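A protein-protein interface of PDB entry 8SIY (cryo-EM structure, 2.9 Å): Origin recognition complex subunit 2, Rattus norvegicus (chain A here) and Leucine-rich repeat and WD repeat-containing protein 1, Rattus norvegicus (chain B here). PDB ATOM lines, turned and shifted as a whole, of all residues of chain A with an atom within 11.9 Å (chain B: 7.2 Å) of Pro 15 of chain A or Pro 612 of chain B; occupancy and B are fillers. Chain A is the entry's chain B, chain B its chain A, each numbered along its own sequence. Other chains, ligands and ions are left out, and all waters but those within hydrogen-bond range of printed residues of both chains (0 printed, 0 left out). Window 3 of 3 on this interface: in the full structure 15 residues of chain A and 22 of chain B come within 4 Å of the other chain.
The backbone carbonyl oxygen (O) of Pro 612 of chain B is in hydrogen-bond range of the backbone NH (N) of Val 619 of chain B, 3.0 Å away.
Of the 6 printed residues of chain A, 4 touch a printed residue of chain B. Hydrophobic or aromatic side chains of chain A that line the printed part of chain B: Pro 15 and Val 17. Among the printed residues, 11 pairs touch across the chains.
Of the printed residues of chain B, Pro 15 of chain A touches Pro 276, Phe 279 and Pro 612. Pro 612 of chain B touches two residues of chain A. No residue of chain A comes within 4 Å of His 278 of chain B. No residue of chain A comes within 4 Å of Trp 609 of chain B. No residue of chain A comes within 4 Å of Gln 611 of chain B. Of chain A, only Ser 16 and Val 17 come within 4 Å of Val 613 of chain B. Of the printed residues of chain A, Ala 614 of chain B touches Val 17 (3.5 Å). Pro 618 of chain B touches none of the printed residues of chain A. No residue of chain A comes within 4 Å of Val 619 of chain B. Of the printed residues of chain B, Gln 18 of chain A touches Phe 279. Of the printed residues of chain A, Ile 644 of chain B touches Val 17. Printed residues of chain B within 4 Å of Val 17 of chain A: Phe 279, Pro 612, Val 613, Ala 614 and Ile 644. Leu 277 of chain B touches none of the printed residues of chain A. The nearest residue of chain A that does not touch Pro 612 of chain B is Val 14 of chain A (4.4 Å). The nearest printed residue of chain B that does not touch Val 17 of chain A is Leu 615 of chain B (4.5 Å).
Among the printed residues, merely in contact across the chains: Pro 15 of chain A with Pro 276 of chain B, Pro 15 of chain A with Phe 279 of chain B, Pro 15 of chain A with Pro 612 of chain B, Ser 16 of chain A with Phe 279 of chain B, Ser 16 of chain A with Val 613 of chain B, Val 17 of chain A with Phe 279 of chain B, Val 17 of chain A with Pro 612 of chain B, Val 17 of chain A with Ala 614 of chain B and Val 17 of chain A with Ile 644 of chain B.
O of Phe 279 of chain B is in hydrogen-bond range of N of Gln 18 of chain A, at 2.6 Å. N of Val 17 of chain A sits at hydrogen-bond distance from O of Val 613 of chain B, at 3.0 Å.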
ATOM      1  N   VAL A  14      -7.741   1.773  -3.856  1.00  0.00           N
ATOM      2  CA  VAL A  14      -7.715   1.302  -2.477  1.00  0.00           C
ATOM      3  C   VAL A  14      -8.590   0.056  -2.341  1.00  0.00           C
ATOM      4  O   VAL A  14      -9.790   0.113  -2.609  1.00  0.00           O
ATOM      5  CB  VAL A  14      -8.180   2.402  -1.507  1.00  0.00           C
ATOM      6  CG1 VAL A  14      -8.215   1.873  -0.080  1.00  0.00           C
ATOM      7  CG2 VAL A  14      -7.269   3.616  -1.608  1.00  0.00           C
ATOM      8  N   PRO A  15      -8.003  -1.069  -1.930  1.00  0.00           N
ATOM      9  CA  PRO A  15      -8.808  -2.284  -1.761  1.00  0.00           C
ATOM     10  C   PRO A  15      -9.928  -2.070  -0.753  1.00  0.00           C
ATOM     11  O   PRO A  15      -9.764  -1.373   0.250  1.00  0.00           O
ATOM     12  CB  PRO A  15      -7.794  -3.319  -1.261  1.00  0.00           C
ATOM     13  CG  PRO A  15      -6.473  -2.810  -1.707  1.00  0.00           C
ATOM     14  CD  PRO A  15      -6.577  -1.320  -1.656  1.00  0.00           C
ATOM     15  N   SER A  16     -11.076  -2.682  -1.030  1.00  0.00           N
ATOM     16  CA  SER A  16     -12.177  -2.682  -0.083  1.00  0.00           C
ATOM     17  C   SER A  16     -11.927  -3.721   1.008  1.00  0.00           C
ATOM     18  O   SER A  16     -11.008  -4.540   0.926  1.00  0.00           O
ATOM     19  CB  SER A  16     -13.496  -2.967  -0.796  1.00  0.00           C
ATOM     20  OG  SER A  16     -13.456  -4.221  -1.454  1.00  0.00           O
ATOM     21  N   VAL A  17     -12.759  -3.684   2.049  1.00  0.00           N
ATOM     22  CA  VAL A  17     -12.612  -4.639   3.137  1.00  0.00           C
ATOM     23  C   VAL A  17     -13.125  -5.995   2.679  1.00  0.00           C
ATOM     24  O   VAL A  17     -14.247  -6.115   2.169  1.00  0.00           O
ATOM     25  CB  VAL A  17     -13.348  -4.154   4.396  1.00  0.00           C
ATOM     26  CG1 VAL A  17     -13.013  -2.695   4.687  1.00  0.00           C
ATOM     27  CG2 VAL A  17     -14.848  -4.354   4.255  1.00  0.00           C
ATOM     28  N   GLN A  18     -12.299  -7.021   2.849  1.00  0.00           N
ATOM     29  CA  GLN A  18     -12.624  -8.378   2.430  1.00  0.00           C
ATOM     30  C   GLN A  18     -13.044  -9.186   3.651  1.00  0.00           C
ATOM     31  O   GLN A  18     -12.255  -9.362   4.584  1.00  0.00           O
ATOM     32  CB  GLN A  18     -11.426  -9.027   1.738  1.00  0.00           C
ATOM     33  CG  GLN A  18     -11.655 -10.465   1.315  1.00  0.00           C
ATOM     34  CD  GLN A  18     -12.768 -10.598   0.298  1.00  0.00           C
ATOM     35  OE1 GLN A  18     -12.777  -9.912  -0.723  1.00  0.00           O
ATOM     36  NE2 GLN A  18     -13.719 -11.482   0.576  1.00  0.00           N
ATOM     37  N   PHE A  19     -14.283  -9.674   3.643  1.00  0.00           N
ATOM     38  CA  PHE A  19     -14.767 -10.526   4.718  1.00  0.00           C
ATOM     39  C   PHE A  19     -14.315 -11.960   4.495  1.00  0.00           C
ATOM     40  O   PHE A  19     -14.364 -12.469   3.372  1.00  0.00           O
ATOM     41  CB  PHE A  19     -16.286 -10.478   4.814  1.00  0.00           C
ATOM     42  CG  PHE A  19     -16.858 -11.541   5.706  1.00  0.00           C
ATOM     43  CD1 PHE A  19     -16.822 -11.399   7.081  1.00  0.00           C
ATOM     44  CD2 PHE A  19     -17.413 -12.690   5.172  1.00  0.00           C
ATOM     45  CE1 PHE A  19     -17.340 -12.376   7.907  1.00  0.00           C
ATOM     46  CE2 PHE A  19     -17.931 -13.671   5.994  1.00  0.00           C
ATOM     47  CZ  PHE A  19     -17.894 -13.513   7.362  1.00  0.00           C
ATOM     48  N   GLU B 275       2.180   0.864   0.087  1.00  0.00           N
ATOM     49  CA  GLU B 275       0.898   0.831  -0.595  1.00  0.00           C
ATOM     50  C   GLU B 275      -0.020  -0.186   0.065  1.00  0.00           C
ATOM     51  O   GLU B 275       0.462  -1.220   0.570  1.00  0.00           O
ATOM     52  CB  GLU B 275       1.055   0.494  -2.087  1.00  0.00           C
ATOM     53  CG  GLU B 275       1.459   1.697  -2.913  1.00  0.00           C
ATOM     54  CD  GLU B 275       0.322   2.694  -3.063  1.00  0.00           C
ATOM     55  OE1 GLU B 275      -0.041   3.345  -2.059  1.00  0.00           O
ATOM     56  OE2 GLU B 275      -0.221   2.820  -4.181  1.00  0.00           O
ATOM     57  N   PRO B 276      -1.339   0.069   0.070  1.00  0.00           N
ATOM     58  CA  PRO B 276      -2.262  -0.871   0.715  1.00  0.00           C
ATOM     59  C   PRO B 276      -2.419  -2.144  -0.101  1.00  0.00           C
ATOM     60  O   PRO B 276      -2.714  -2.093  -1.296  1.00  0.00           O
ATOM     61  CB  PRO B 276      -3.578  -0.076   0.787  1.00  0.00           C
ATOM     62  CG  PRO B 276      -3.433   1.071  -0.226  1.00  0.00           C
ATOM     63  CD  PRO B 276      -1.991   1.382  -0.122  1.00  0.00           C
ATOM     64  N   LEU B 277      -2.239  -3.290   0.559  1.00  0.00           N
ATOM     65  CA  LEU B 277      -2.311  -4.599  -0.085  1.00  0.00           C
ATOM     66  C   LEU B 277      -3.538  -5.423   0.302  1.00  0.00           C
ATOM     67  O   LEU B 277      -4.073  -6.136  -0.546  1.00  0.00           O
ATOM     68  CB  LEU B 277      -1.047  -5.424   0.212  1.00  0.00           C
ATOM     69  CG  LEU B 277      -0.479  -6.278  -0.954  1.00  0.00           C
ATOM     70  CD1 LEU B 277       0.878  -6.890  -0.591  1.00  0.00           C
ATOM     71  CD2 LEU B 277      -1.399  -7.422  -1.394  1.00  0.00           C
ATOM     72  N   HIS B 278      -3.998  -5.385   1.559  1.00  0.00           N
ATOM     73  CA  HIS B 278      -5.234  -6.074   1.927  1.00  0.00           C
ATOM     74  C   HIS B 278      -5.947  -5.337   3.049  1.00  0.00           C
ATOM     75  O   HIS B 278      -5.326  -4.621   3.838  1.00  0.00           O
ATOM     76  CB  HIS B 278      -5.002  -7.529   2.383  1.00  0.00           C
ATOM     77  CG  HIS B 278      -4.479  -8.428   1.308  1.00  0.00           C
ATOM     78  ND1 HIS B 278      -5.241  -8.827   0.226  1.00  0.00           N
ATOM     79  CD2 HIS B 278      -3.291  -9.064   1.184  1.00  0.00           C
ATOM     80  CE1 HIS B 278      -4.525  -9.630  -0.541  1.00  0.00           C
ATOM     81  NE2 HIS B 278      -3.343  -9.797   0.024  1.00  0.00           N
ATOM     82  N   PHE B 279      -7.263  -5.525   3.110  1.00  0.00           N
ATOM     83  CA  PHE B 279      -8.078  -5.159   4.266  1.00  0.00           C
ATOM     84  C   PHE B 279      -8.987  -6.350   4.550  1.00  0.00           C
ATOM     85  O   PHE B 279     -10.015  -6.521   3.889  1.00  0.00           O
ATOM     86  CB  PHE B 279      -8.875  -3.885   4.014  1.00  0.00           C
ATOM     87  CG  PHE B 279      -8.019  -2.664   3.825  1.00  0.00           C
ATOM     88  CD1 PHE B 279      -7.598  -1.922   4.916  1.00  0.00           C
ATOM     89  CD2 PHE B 279      -7.633  -2.261   2.559  1.00  0.00           C
ATOM     90  CE1 PHE B 279      -6.811  -0.800   4.746  1.00  0.00           C
ATOM     91  CE2 PHE B 279      -6.845  -1.138   2.384  1.00  0.00           C
ATOM     92  CZ  PHE B 279      -6.433  -0.407   3.479  1.00  0.00           C
ATOM     93  N   TRP B 609      -5.325   6.869   7.332  1.00  0.00           N
ATOM     94  CA  TRP B 609      -6.307   5.798   7.224  1.00  0.00           C
ATOM     95  C   TRP B 609      -7.044   5.921   5.896  1.00  0.00           C
ATOM     96  O   TRP B 609      -7.908   6.793   5.750  1.00  0.00           O
ATOM     97  CB  TRP B 609      -7.276   5.867   8.407  1.00  0.00           C
ATOM     98  CG  TRP B 609      -8.415   4.897   8.347  1.00  0.00           C
ATOM     99  CD1 TRP B 609      -9.743   5.202   8.335  1.00  0.00           C
ATOM    100  CD2 TRP B 609      -8.332   3.468   8.312  1.00  0.00           C
ATOM    101  NE1 TRP B 609     -10.494   4.053   8.287  1.00  0.00           N
ATOM    102  CE2 TRP B 609      -9.650   2.974   8.269  1.00  0.00           C
ATOM    103  CE3 TRP B 609      -7.271   2.557   8.300  1.00  0.00           C
ATOM    104  CZ2 TRP B 609      -9.938   1.613   8.221  1.00  0.00           C
ATOM    105  CZ3 TRP B 609      -7.559   1.206   8.253  1.00  0.00           C
ATOM    106  CH2 TRP B 609      -8.881   0.747   8.215  1.00  0.00           C
ATOM    107  N   PRO B 610      -6.764   5.061   4.917  1.00  0.00           N
ATOM    108  CA  PRO B 610      -7.302   5.260   3.568  1.00  0.00           C
ATOM    109  C   PRO B 610      -8.807   5.084   3.444  1.00  0.00           C
ATOM    110  O   PRO B 610      -9.317   5.113   2.320  1.00  0.00           O
ATOM    111  CB  PRO B 610      -6.560   4.190   2.750  1.00  0.00           C
ATOM    112  CG  PRO B 610      -6.239   3.132   3.729  1.00  0.00           C
ATOM    113  CD  PRO B 610      -5.913   3.860   4.990  1.00  0.00           C
ATOM    114  N   GLN B 611      -9.526   4.906   4.545  1.00  0.00           N
ATOM    115  CA  GLN B 611     -10.987   4.819   4.532  1.00  0.00           C
ATOM    116  C   GLN B 611     -11.487   3.763   3.550  1.00  0.00           C
ATOM    117  O   GLN B 611     -12.271   4.079   2.641  1.00  0.00           O
ATOM    118  CB  GLN B 611     -11.588   6.176   4.215  1.00  0.00           C
ATOM    119  CG  GLN B 611     -10.835   7.349   4.811  1.00  0.00           C
ATOM    120  CD  GLN B 611     -11.695   8.590   4.936  1.00  0.00           C
ATOM    121  OE1 GLN B 611     -12.902   8.503   5.158  1.00  0.00           O
ATOM    122  NE2 GLN B 611     -11.077   9.757   4.793  1.00  0.00           N
ATOM    123  N   PRO B 612     -11.074   2.507   3.691  1.00  0.00           N
ATOM    124  CA  PRO B 612     -11.535   1.482   2.750  1.00  0.00           C
ATOM    125  C   PRO B 612     -13.041   1.299   2.843  1.00  0.00           C
ATOM    126  O   PRO B 612     -13.655   1.519   3.888  1.00  0.00           O
ATOM    127  CB  PRO B 612     -10.788   0.219   3.194  1.00  0.00           C
ATOM    128  CG  PRO B 612      -9.659   0.701   4.022  1.00  0.00           C
ATOM    129  CD  PRO B 612     -10.129   1.956   4.676  1.00  0.00           C
ATOM    130  N   VAL B 613     -13.633   0.892   1.728  1.00  0.00           N
ATOM    131  CA  VAL B 613     -15.080   0.729   1.649  1.00  0.00           C
ATOM    132  C   VAL B 613     -15.477  -0.569   2.338  1.00  0.00           C
ATOM    133  O   VAL B 613     -14.902  -1.631   2.070  1.00  0.00           O
ATOM    134  CB  VAL B 613     -15.544   0.741   0.185  1.00  0.00           C
ATOM    135  CG1 VAL B 613     -16.995   0.302   0.087  1.00  0.00           C
ATOM    136  CG2 VAL B 613     -15.356   2.123  -0.419  1.00  0.00           C
ATOM    137  N   ALA B 614     -16.461  -0.486   3.233  1.00  0.00           N
ATOM    138  CA  ALA B 614     -17.010  -1.645   3.923  1.00  0.00           C
ATOM    139  C   ALA B 614     -18.513  -1.694   3.699  1.00  0.00           C
ATOM    140  O   ALA B 614     -19.215  -0.712   3.959  1.00  0.00           O
ATOM    141  CB  ALA B 614     -16.701  -1.596   5.421  1.00  0.00           C
ATOM    142  N   LEU B 615     -19.003  -2.841   3.227  1.00  0.00           N
ATOM    143  CA  LEU B 615     -20.420  -3.017   2.919  1.00  0.00           C
ATOM    144  C   LEU B 615     -20.909  -1.960   1.934  1.00  0.00           C
ATOM    145  O   LEU B 615     -22.076  -1.559   1.963  1.00  0.00           O
ATOM    146  CB  LEU B 615     -21.272  -2.988   4.194  1.00  0.00           C
ATOM    147  CG  LEU B 615     -20.980  -4.066   5.241  1.00  0.00           C
ATOM    148  CD1 LEU B 615     -21.809  -3.827   6.494  1.00  0.00           C
ATOM    149  CD2 LEU B 615     -21.245  -5.457   4.685  1.00  0.00           C
ATOM    150  N   GLN B 617     -19.743   1.145   1.821  1.00  0.00           N
ATOM    151  CA  GLN B 617     -19.540   2.469   2.386  1.00  0.00           C
ATOM    152  C   GLN B 617     -18.135   2.587   2.969  1.00  0.00           C
ATOM    153  O   GLN B 617     -17.540   1.580   3.361  1.00  0.00           O
ATOM    154  CB  GLN B 617     -20.572   2.762   3.483  1.00  0.00           C
ATOM    155  CG  GLN B 617     -22.016   2.722   3.002  1.00  0.00           C
ATOM    156  CD  GLN B 617     -22.867   1.723   3.767  1.00  0.00           C
ATOM    157  OE1 GLN B 617     -22.785   1.627   4.990  1.00  0.00           O
ATOM    158  NE2 GLN B 617     -23.687   0.969   3.043  1.00  0.00           N
ATOM    159  N   PRO B 618     -17.571   3.794   3.023  1.00  0.00           N
ATOM    160  CA  PRO B 618     -16.251   3.960   3.647  1.00  0.00           C
ATOM    161  C   PRO B 618     -16.317   3.868   5.165  1.00  0.00           C
ATOM    162  O   PRO B 618     -17.242   4.381   5.799  1.00  0.00           O
ATOM    163  CB  PRO B 618     -15.818   5.359   3.194  1.00  0.00           C
ATOM    164  CG  PRO B 618     -17.092   6.083   2.949  1.00  0.00           C
ATOM    165  CD  PRO B 618     -18.069   5.055   2.446  1.00  0.00           C
ATOM    166  N   VAL B 619     -15.315   3.209   5.744  1.00  0.00           N
ATOM    167  CA  VAL B 619     -15.141   3.162   7.199  1.00  0.00           C
ATOM    168  C   VAL B 619     -14.332   4.402   7.563  1.00  0.00           C
ATOM    169  O   VAL B 619     -13.102   4.383   7.610  1.00  0.00           O
ATOM    170  CB  VAL B 619     -14.467   1.871   7.653  1.00  0.00           C
ATOM    171  CG1 VAL B 619     -14.300   1.857   9.167  1.00  0.00           C
ATOM    172  CG2 VAL B 619     -15.270   0.669   7.187  1.00  0.00           C
ATOM    173  N   THR B 620     -15.040   5.498   7.830  1.00  0.00           N
ATOM    174  CA  THR B 620     -14.397   6.804   7.930  1.00  0.00           C
ATOM    175  C   THR B 620     -13.607   6.986   9.220  1.00  0.00           C
ATOM    176  O   THR B 620     -12.620   7.730   9.229  1.00  0.00           O
ATOM    177  CB  THR B 620     -15.451   7.908   7.818  1.00  0.00           C
ATOM    178  OG1 THR B 620     -16.482   7.685   8.788  1.00  0.00           O
ATOM    179  CG2 THR B 620     -16.059   7.917   6.426  1.00  0.00           C
ATOM    180  N   ILE B 644     -10.490  -5.142  11.164  1.00  0.00           N
ATOM    181  CA  ILE B 644      -9.852  -5.035   9.860  1.00  0.00           C
ATOM    182  C   ILE B 644      -8.358  -5.196  10.067  1.00  0.00           C
ATOM    183  O   ILE B 644      -7.748  -4.426  10.818  1.00  0.00           O
ATOM    184  CB  ILE B 644     -10.151  -3.692   9.179  1.00  0.00           C
ATOM    185  CG1 ILE B 644     -11.641  -3.584   8.848  1.00  0.00           C
ATOM    186  CG2 ILE B 644      -9.291  -3.533   7.935  1.00  0.00           C
ATOM    187  CD1 ILE B 644     -12.089  -2.181   8.499  1.00  0.00           C
ATOM    188  N   SER B 646      -5.315  -4.348   8.491  1.00  0.00           N
ATOM    189  CA  SER B 646      -4.732  -3.518   7.450  1.00  0.00           C
ATOM    190  C   SER B 646      -3.353  -4.051   7.109  1.00  0.00           C
ATOM    191  O   SER B 646      -2.493  -4.171   7.986  1.00  0.00           O
ATOM    192  CB  SER B 646      -4.633  -2.065   7.914  1.00  0.00           C
ATOM    193  OG  SER B 646      -5.895  -1.558   8.307  1.00  0.00           O
ATOM    194  N   ILE B 647      -3.134  -4.366   5.838  1.00  0.00           N
ATOM    195  CA  ILE B 647      -1.850  -4.867   5.369  1.00  0.00           C
ATOM    196  C   ILE B 647      -1.307  -3.893   4.336  1.00  0.00           C
ATOM    197  O   ILE B 647      -2.019  -3.504   3.404  1.00  0.00           O
ATOM    198  CB  ILE B 647      -1.965  -6.290   4.790  1.00  0.00           C
ATOM    199  CG1 ILE B 647      -2.345  -7.277   5.899  1.00  0.00           C
ATOM    200  CG2 ILE B 647      -0.645  -6.702   4.154  1.00  0.00           C
ATOM    201  CD1 ILE B 647      -2.843  -8.627   5.402  1.00  0.00           C
